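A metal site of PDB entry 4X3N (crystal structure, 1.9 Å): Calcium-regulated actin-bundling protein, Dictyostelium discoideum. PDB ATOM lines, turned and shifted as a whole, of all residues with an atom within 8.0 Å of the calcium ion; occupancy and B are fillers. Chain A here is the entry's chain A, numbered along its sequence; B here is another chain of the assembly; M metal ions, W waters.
The guanidinium group (NE) of Arg 150 lies within salt-bridge range of the side-chain carboxylate (OD1) of Asp 93 (2.7 Å).
The side-chain carboxylate of Asp 144 sits close to the backbone NH of Phe 147 (3.4 Å).
The side-chain carboxylate (OD2) of Asp 144 sits at hydrogen-bond distance from the backbone NH (N) of Gly 149 (2.8 Å).
The side-chain hydroxyl of Tyr 101 of chain B lies within hydrogen-bond range of the side-chain carboxylate of Asp 144 (2.6 Å).
O of Leu 139 sits at hydrogen-bond distance from N of Asp 144 (2.7 Å).
ND2 of Asn 146 lies within hydrogen-bond range of SG of Cys 35, 3.5 Å away.
The backbone NH of Val 145 lies close to the side-chain carboxylate of Glu 155, 3.0 Å away.
The backbone NH (N) of Glu 155 lies within hydrogen-bond range of the side-chain hydroxyl (OG) of Ser 152 (3.0 Å).
The nearest printed residue that does not touch the calcium ion is Val 151 (4.4 Å).
The calcium ion is bound by O of Arg 150 (2.3 Å), OD1 of Asp 144 (2.3 Å), water W1 (2.4 Å), OD1 of Asn 146 (2.4 Å), OD1 of Asp 148 (2.5 Å), OE2 of Glu 155 (2.5 Å) and OE1 of Glu 155 (2.6 Å).
The calcium ion has seven donor atoms within binding distance.
Water W1 bridges OD2 of Asp 148 (2.6 Å) and ND2 of Asn 146 (3.1 Å).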
ATOM      1  N   PHE A  34      -1.226  20.281  21.264  1.00  0.00           N
ATOM      2  CA  PHE A  34      -2.245  21.224  20.860  1.00  0.00           C
ATOM      3  C   PHE A  34      -3.239  20.554  19.935  1.00  0.00           C
ATOM      4  O   PHE A  34      -4.444  20.710  20.109  1.00  0.00           O
ATOM      5  CB  PHE A  34      -1.552  22.362  20.102  1.00  0.00           C
ATOM      6  CG  PHE A  34      -2.438  23.509  19.775  1.00  0.00           C
ATOM      7  CD1 PHE A  34      -3.156  23.519  18.657  1.00  0.00           C
ATOM      8  CD2 PHE A  34      -2.457  24.626  20.602  1.00  0.00           C
ATOM      9  CE1 PHE A  34      -3.997  24.597  18.358  1.00  0.00           C
ATOM     10  CE2 PHE A  34      -3.288  25.704  20.332  1.00  0.00           C
ATOM     11  CZ  PHE A  34      -4.045  25.702  19.206  1.00  0.00           C
ATOM     12  N   CYS A  35      -2.756  19.851  18.941  1.00  0.00           N
ATOM     13  CA  CYS A  35      -3.655  19.198  17.994  1.00  0.00           C
ATOM     14  C   CYS A  35      -4.552  18.193  18.691  1.00  0.00           C
ATOM     15  O   CYS A  35      -5.755  18.080  18.331  1.00  0.00           O
ATOM     16  CB  CYS A  35      -2.894  18.538  16.820  1.00  0.00           C
ATOM     17  SG  CYS A  35      -2.202  19.785  15.711  1.00  0.00           S
ATOM     18  N   ALA A  38      -7.194  20.039  20.657  1.00  0.00           N
ATOM     19  CA  ALA A  38      -8.117  20.641  19.732  1.00  0.00           C
ATOM     20  C   ALA A  38      -9.076  19.633  19.014  1.00  0.00           C
ATOM     21  O   ALA A  38     -10.089  20.025  18.473  1.00  0.00           O
ATOM     22  CB  ALA A  38      -7.383  21.516  18.713  1.00  0.00           C
ATOM     23  N   LYS A  39      -8.783  18.346  19.070  1.00  0.00           N
ATOM     24  CA  LYS A  39      -9.696  17.318  18.569  1.00  0.00           C
ATOM     25  C   LYS A  39     -10.596  16.743  19.638  1.00  0.00           C
ATOM     26  O   LYS A  39     -11.442  15.945  19.321  1.00  0.00           O
ATOM     27  CB  LYS A  39      -8.923  16.183  17.930  1.00  0.00           C
ATOM     28  CG  LYS A  39      -8.300  16.601  16.610  1.00  0.00           C
ATOM     29  CD  LYS A  39      -9.381  16.831  15.536  1.00  0.00           C
ATOM     30  CE  LYS A  39      -8.801  17.055  14.140  1.00  0.00           C
ATOM     31  NZ  LYS A  39      -9.912  17.461  13.198  1.00  0.00           N
ATOM     32  N   ASP A  93     -14.245  20.753  15.803  1.00  0.00           N
ATOM     33  CA  ASP A  93     -13.801  21.901  15.002  1.00  0.00           C
ATOM     34  C   ASP A  93     -14.715  22.150  13.765  1.00  0.00           C
ATOM     35  O   ASP A  93     -15.590  21.379  13.436  1.00  0.00           O
ATOM     36  CB  ASP A  93     -12.364  21.755  14.739  1.00  0.00           C
ATOM     37  CG  ASP A  93     -12.013  20.552  13.801  1.00  0.00           C
ATOM     38  OD1 ASP A  93     -12.806  20.212  12.927  1.00  0.00           O
ATOM     39  OD2 ASP A  93     -11.008  19.914  14.023  1.00  0.00           O
ATOM     40  N   LEU A  94     -14.549  23.310  13.165  1.00  0.00           N
ATOM     41  CA  LEU A  94     -15.367  23.800  12.090  1.00  0.00           C
ATOM     42  C   LEU A  94     -14.479  24.157  10.861  1.00  0.00           C
ATOM     43  O   LEU A  94     -13.377  24.723  10.991  1.00  0.00           O
ATOM     44  CB  LEU A  94     -16.087  25.087  12.507  1.00  0.00           C
ATOM     45  CG  LEU A  94     -16.779  25.155  13.893  1.00  0.00           C
ATOM     46  CD1 LEU A  94     -17.414  26.542  14.067  1.00  0.00           C
ATOM     47  CD2 LEU A  94     -17.813  24.041  14.005  1.00  0.00           C
ATOM     48  N   PHE A  96     -13.862  26.590   7.533  1.00  0.00           N
ATOM     49  CA  PHE A  96     -13.919  28.045   7.530  1.00  0.00           C
ATOM     50  C   PHE A  96     -15.322  28.639   7.191  1.00  0.00           C
ATOM     51  O   PHE A  96     -15.729  29.738   7.685  1.00  0.00           O
ATOM     52  CB  PHE A  96     -12.847  28.625   6.582  1.00  0.00           C
ATOM     53  CG  PHE A  96     -11.432  28.593   7.105  1.00  0.00           C
ATOM     54  CD1 PHE A  96     -11.081  28.034   8.298  1.00  0.00           C
ATOM     55  CD2 PHE A  96     -10.430  29.099   6.298  1.00  0.00           C
ATOM     56  CE1 PHE A  96      -9.773  27.994   8.699  1.00  0.00           C
ATOM     57  CE2 PHE A  96      -9.109  29.076   6.695  1.00  0.00           C
ATOM     58  CZ  PHE A  96      -8.782  28.525   7.906  1.00  0.00           C
ATOM     59  N   LEU A 139      -9.036  34.127  10.096  1.00  0.00           N
ATOM     60  CA  LEU A 139      -8.954  32.681  10.460  1.00  0.00           C
ATOM     61  C   LEU A 139      -7.623  32.131  10.030  1.00  0.00           C
ATOM     62  O   LEU A 139      -6.936  31.450  10.762  1.00  0.00           O
ATOM     63  CB  LEU A 139     -10.099  31.883   9.768  1.00  0.00           C
ATOM     64  CG  LEU A 139     -11.532  32.267  10.152  1.00  0.00           C
ATOM     65  CD1 LEU A 139     -12.506  31.266   9.576  1.00  0.00           C
ATOM     66  CD2 LEU A 139     -11.734  32.369  11.645  1.00  0.00           C
ATOM     67  N   VAL A 143      -6.246  32.716  13.563  1.00  0.00           N
ATOM     68  CA  VAL A 143      -6.988  31.784  14.407  1.00  0.00           C
ATOM     69  C   VAL A 143      -6.546  30.365  14.204  1.00  0.00           C
ATOM     70  O   VAL A 143      -6.422  29.612  15.193  1.00  0.00           O
ATOM     71  CB  VAL A 143      -8.502  31.895  14.243  1.00  0.00           C
ATOM     72  CG1 VAL A 143      -9.264  30.935  15.179  1.00  0.00           C
ATOM     73  CG2 VAL A 143      -8.964  33.331  14.474  1.00  0.00           C
ATOM     74  N   ASP A 144      -6.363  29.981  12.936  1.00  0.00           N
ATOM     75  CA  ASP A 144      -5.983  28.584  12.595  1.00  0.00           C
ATOM     76  C   ASP A 144      -4.505  28.286  12.764  1.00  0.00           C
ATOM     77  O   ASP A 144      -3.743  28.095  11.749  1.00  0.00           O
ATOM     78  CB  ASP A 144      -6.449  28.239  11.176  1.00  0.00           C
ATOM     79  CG  ASP A 144      -6.153  26.784  10.791  1.00  0.00           C
ATOM     80  OD1 ASP A 144      -6.020  25.936  11.684  1.00  0.00           O
ATOM     81  OD2 ASP A 144      -6.080  26.533   9.578  1.00  0.00           O
ATOM     82  N   VAL A 145      -4.117  28.108  14.031  1.00  0.00           N
ATOM     83  CA  VAL A 145      -2.728  28.024  14.385  1.00  0.00           C
ATOM     84  C   VAL A 145      -2.054  26.695  14.058  1.00  0.00           C
ATOM     85  O   VAL A 145      -0.860  26.677  13.906  1.00  0.00           O
ATOM     86  CB  VAL A 145      -2.464  28.437  15.828  1.00  0.00           C
ATOM     87  CG1 VAL A 145      -3.106  29.827  16.110  1.00  0.00           C
ATOM     88  CG2 VAL A 145      -2.959  27.398  16.780  1.00  0.00           C
ATOM     89  N   ASN A 146      -2.792  25.616  13.858  1.00  0.00           N
ATOM     90  CA  ASN A 146      -2.149  24.413  13.371  1.00  0.00           C
ATOM     91  C   ASN A 146      -2.292  24.193  11.882  1.00  0.00           C
ATOM     92  O   ASN A 146      -1.963  23.122  11.392  1.00  0.00           O
ATOM     93  CB  ASN A 146      -2.611  23.215  14.157  1.00  0.00           C
ATOM     94  CG  ASN A 146      -4.099  23.101  14.180  1.00  0.00           C
ATOM     95  OD1 ASN A 146      -4.779  23.858  13.506  1.00  0.00           O
ATOM     96  ND2 ASN A 146      -4.605  22.195  14.995  1.00  0.00           N
ATOM     97  N   PHE A 147      -2.798  25.184  11.155  1.00  0.00           N
ATOM     98  CA  PHE A 147      -2.893  25.162   9.687  1.00  0.00           C
ATOM     99  C   PHE A 147      -3.648  23.996   9.083  1.00  0.00           C
ATOM    100  O   PHE A 147      -3.215  23.425   8.061  1.00  0.00           O
ATOM    101  CB  PHE A 147      -1.495  25.300   9.082  1.00  0.00           C
ATOM    102  CG  PHE A 147      -0.820  26.594   9.446  1.00  0.00           C
ATOM    103  CD1 PHE A 147      -0.008  26.662  10.521  1.00  0.00           C
ATOM    104  CD2 PHE A 147      -1.008  27.716   8.693  1.00  0.00           C
ATOM    105  CE1 PHE A 147       0.621  27.851  10.862  1.00  0.00           C
ATOM    106  CE2 PHE A 147      -0.398  28.919   9.029  1.00  0.00           C
ATOM    107  CZ  PHE A 147       0.427  28.975  10.121  1.00  0.00           C
ATOM    108  N   ASP A 148      -4.788  23.647   9.711  1.00  0.00           N
ATOM    109  CA  ASP A 148      -5.540  22.512   9.221  1.00  0.00           C
ATOM    110  C   ASP A 148      -6.783  22.927   8.493  1.00  0.00           C
ATOM    111  O   ASP A 148      -7.539  22.080   8.093  1.00  0.00           O
ATOM    112  CB  ASP A 148      -5.782  21.451  10.331  1.00  0.00           C
ATOM    113  CG  ASP A 148      -6.713  21.946  11.418  1.00  0.00           C
ATOM    114  OD1 ASP A 148      -7.100  23.098  11.344  1.00  0.00           O
ATOM    115  OD2 ASP A 148      -7.045  21.196  12.340  1.00  0.00           O
ATOM    116  N   GLY A 149      -6.977  24.229   8.298  1.00  0.00           N
ATOM    117  CA  GLY A 149      -8.193  24.798   7.726  1.00  0.00           C
ATOM    118  C   GLY A 149      -9.447  24.614   8.601  1.00  0.00           C
ATOM    119  O   GLY A 149     -10.574  24.717   8.105  1.00  0.00           O
ATOM    120  N   ARG A 150      -9.248  24.274   9.883  1.00  0.00           N
ATOM    121  CA  ARG A 150     -10.334  24.077  10.816  1.00  0.00           C
ATOM    122  C   ARG A 150     -10.191  25.022  12.035  1.00  0.00           C
ATOM    123  O   ARG A 150      -9.056  25.411  12.433  1.00  0.00           O
ATOM    124  CB  ARG A 150     -10.350  22.648  11.329  1.00  0.00           C
ATOM    125  CG  ARG A 150     -10.236  21.512  10.312  1.00  0.00           C
ATOM    126  CD  ARG A 150     -11.476  21.278   9.482  1.00  0.00           C
ATOM    127  NE  ARG A 150     -12.631  20.898  10.285  1.00  0.00           N
ATOM    128  CZ  ARG A 150     -13.804  20.538   9.783  1.00  0.00           C
ATOM    129  NH1 ARG A 150     -13.970  20.493   8.446  1.00  0.00           N
ATOM    130  NH2 ARG A 150     -14.820  20.230  10.590  1.00  0.00           N
ATOM    131  N   VAL A 151     -11.323  25.426  12.591  1.00  0.00           N
ATOM    132  CA  VAL A 151     -11.362  26.225  13.801  1.00  0.00           C
ATOM    133  C   VAL A 151     -11.982  25.400  14.960  1.00  0.00           C
ATOM    134  O   VAL A 151     -13.131  24.950  14.864  1.00  0.00           O
ATOM    135  CB  VAL A 151     -12.131  27.524  13.611  1.00  0.00           C
ATOM    136  CG1 VAL A 151     -12.186  28.283  14.901  1.00  0.00           C
ATOM    137  CG2 VAL A 151     -11.482  28.393  12.536  1.00  0.00           C
ATOM    138  N   SER A 152     -11.151  25.168  15.972  1.00  0.00           N
ATOM    139  CA  SER A 152     -11.539  24.510  17.175  1.00  0.00           C
ATOM    140  C   SER A 152     -12.044  25.577  18.147  1.00  0.00           C
ATOM    141  O   SER A 152     -11.789  26.757  17.959  1.00  0.00           O
ATOM    142  CB  SER A 152     -10.356  23.795  17.761  1.00  0.00           C
ATOM    143  OG  SER A 152      -9.292  24.710  17.991  1.00  0.00           O
ATOM    144  N   GLU A 155      -9.017  27.196  19.574  1.00  0.00           N
ATOM    145  CA  GLU A 155      -8.411  28.231  18.732  1.00  0.00           C
ATOM    146  C   GLU A 155      -9.216  29.535  18.818  1.00  0.00           C
ATOM    147  O   GLU A 155      -8.632  30.588  18.934  1.00  0.00           O
ATOM    148  CB  GLU A 155      -8.264  27.715  17.299  1.00  0.00           C
ATOM    149  CG  GLU A 155      -7.116  26.751  17.163  1.00  0.00           C
ATOM    150  CD  GLU A 155      -7.155  26.032  15.850  1.00  0.00           C
ATOM    151  OE1 GLU A 155      -8.145  25.345  15.600  1.00  0.00           O
ATOM    152  OE2 GLU A 155      -6.195  26.179  15.066  1.00  0.00           O
ATOM    153  N   HIS B  78      -0.145  19.017   8.035  1.00  0.00           N
ATOM    154  CA  HIS B  78      -0.886  19.874   8.954  1.00  0.00           C
ATOM    155  C   HIS B  78      -2.397  19.680   8.839  1.00  0.00           C
ATOM    156  O   HIS B  78      -3.092  19.709   9.825  1.00  0.00           O
ATOM    157  CB  HIS B  78      -0.491  21.339   8.735  1.00  0.00           C
ATOM    158  CG  HIS B  78       0.966  21.595   8.931  1.00  0.00           C
ATOM    159  ND1 HIS B  78       1.620  22.693   8.409  1.00  0.00           N
ATOM    160  CD2 HIS B  78       1.908  20.835   9.546  1.00  0.00           C
ATOM    161  CE1 HIS B  78       2.906  22.629   8.733  1.00  0.00           C
ATOM    162  NE2 HIS B  78       3.109  21.484   9.387  1.00  0.00           N
ATOM    163  N   TYR B 101      -2.404  27.740   1.930  1.00  0.00           N
ATOM    164  CA  TYR B 101      -1.329  27.652   2.877  1.00  0.00           C
ATOM    165  C   TYR B 101      -0.055  27.111   2.202  1.00  0.00           C
ATOM    166  O   TYR B 101       1.051  27.581   2.513  1.00  0.00           O
ATOM    167  CB  TYR B 101      -1.647  26.740   4.062  1.00  0.00           C
ATOM    168  CG  TYR B 101      -2.657  27.216   5.092  1.00  0.00           C
ATOM    169  CD1 TYR B 101      -2.651  28.559   5.556  1.00  0.00           C
ATOM    170  CD2 TYR B 101      -3.513  26.317   5.699  1.00  0.00           C
ATOM    171  CE1 TYR B 101      -3.520  28.967   6.540  1.00  0.00           C
ATOM    172  CE2 TYR B 101      -4.422  26.744   6.675  1.00  0.00           C
ATOM    173  CZ  TYR B 101      -4.401  28.069   7.103  1.00  0.00           C
ATOM    174  OH  TYR B 101      -5.246  28.556   8.097  1.00  0.00           O
HETATM  175 CA    CA M   1      -7.064  24.613  13.295  1.00  0.00          CA
HETATM  176  O   HOH W   1      -7.611  22.619  14.476  1.00  0.00           O
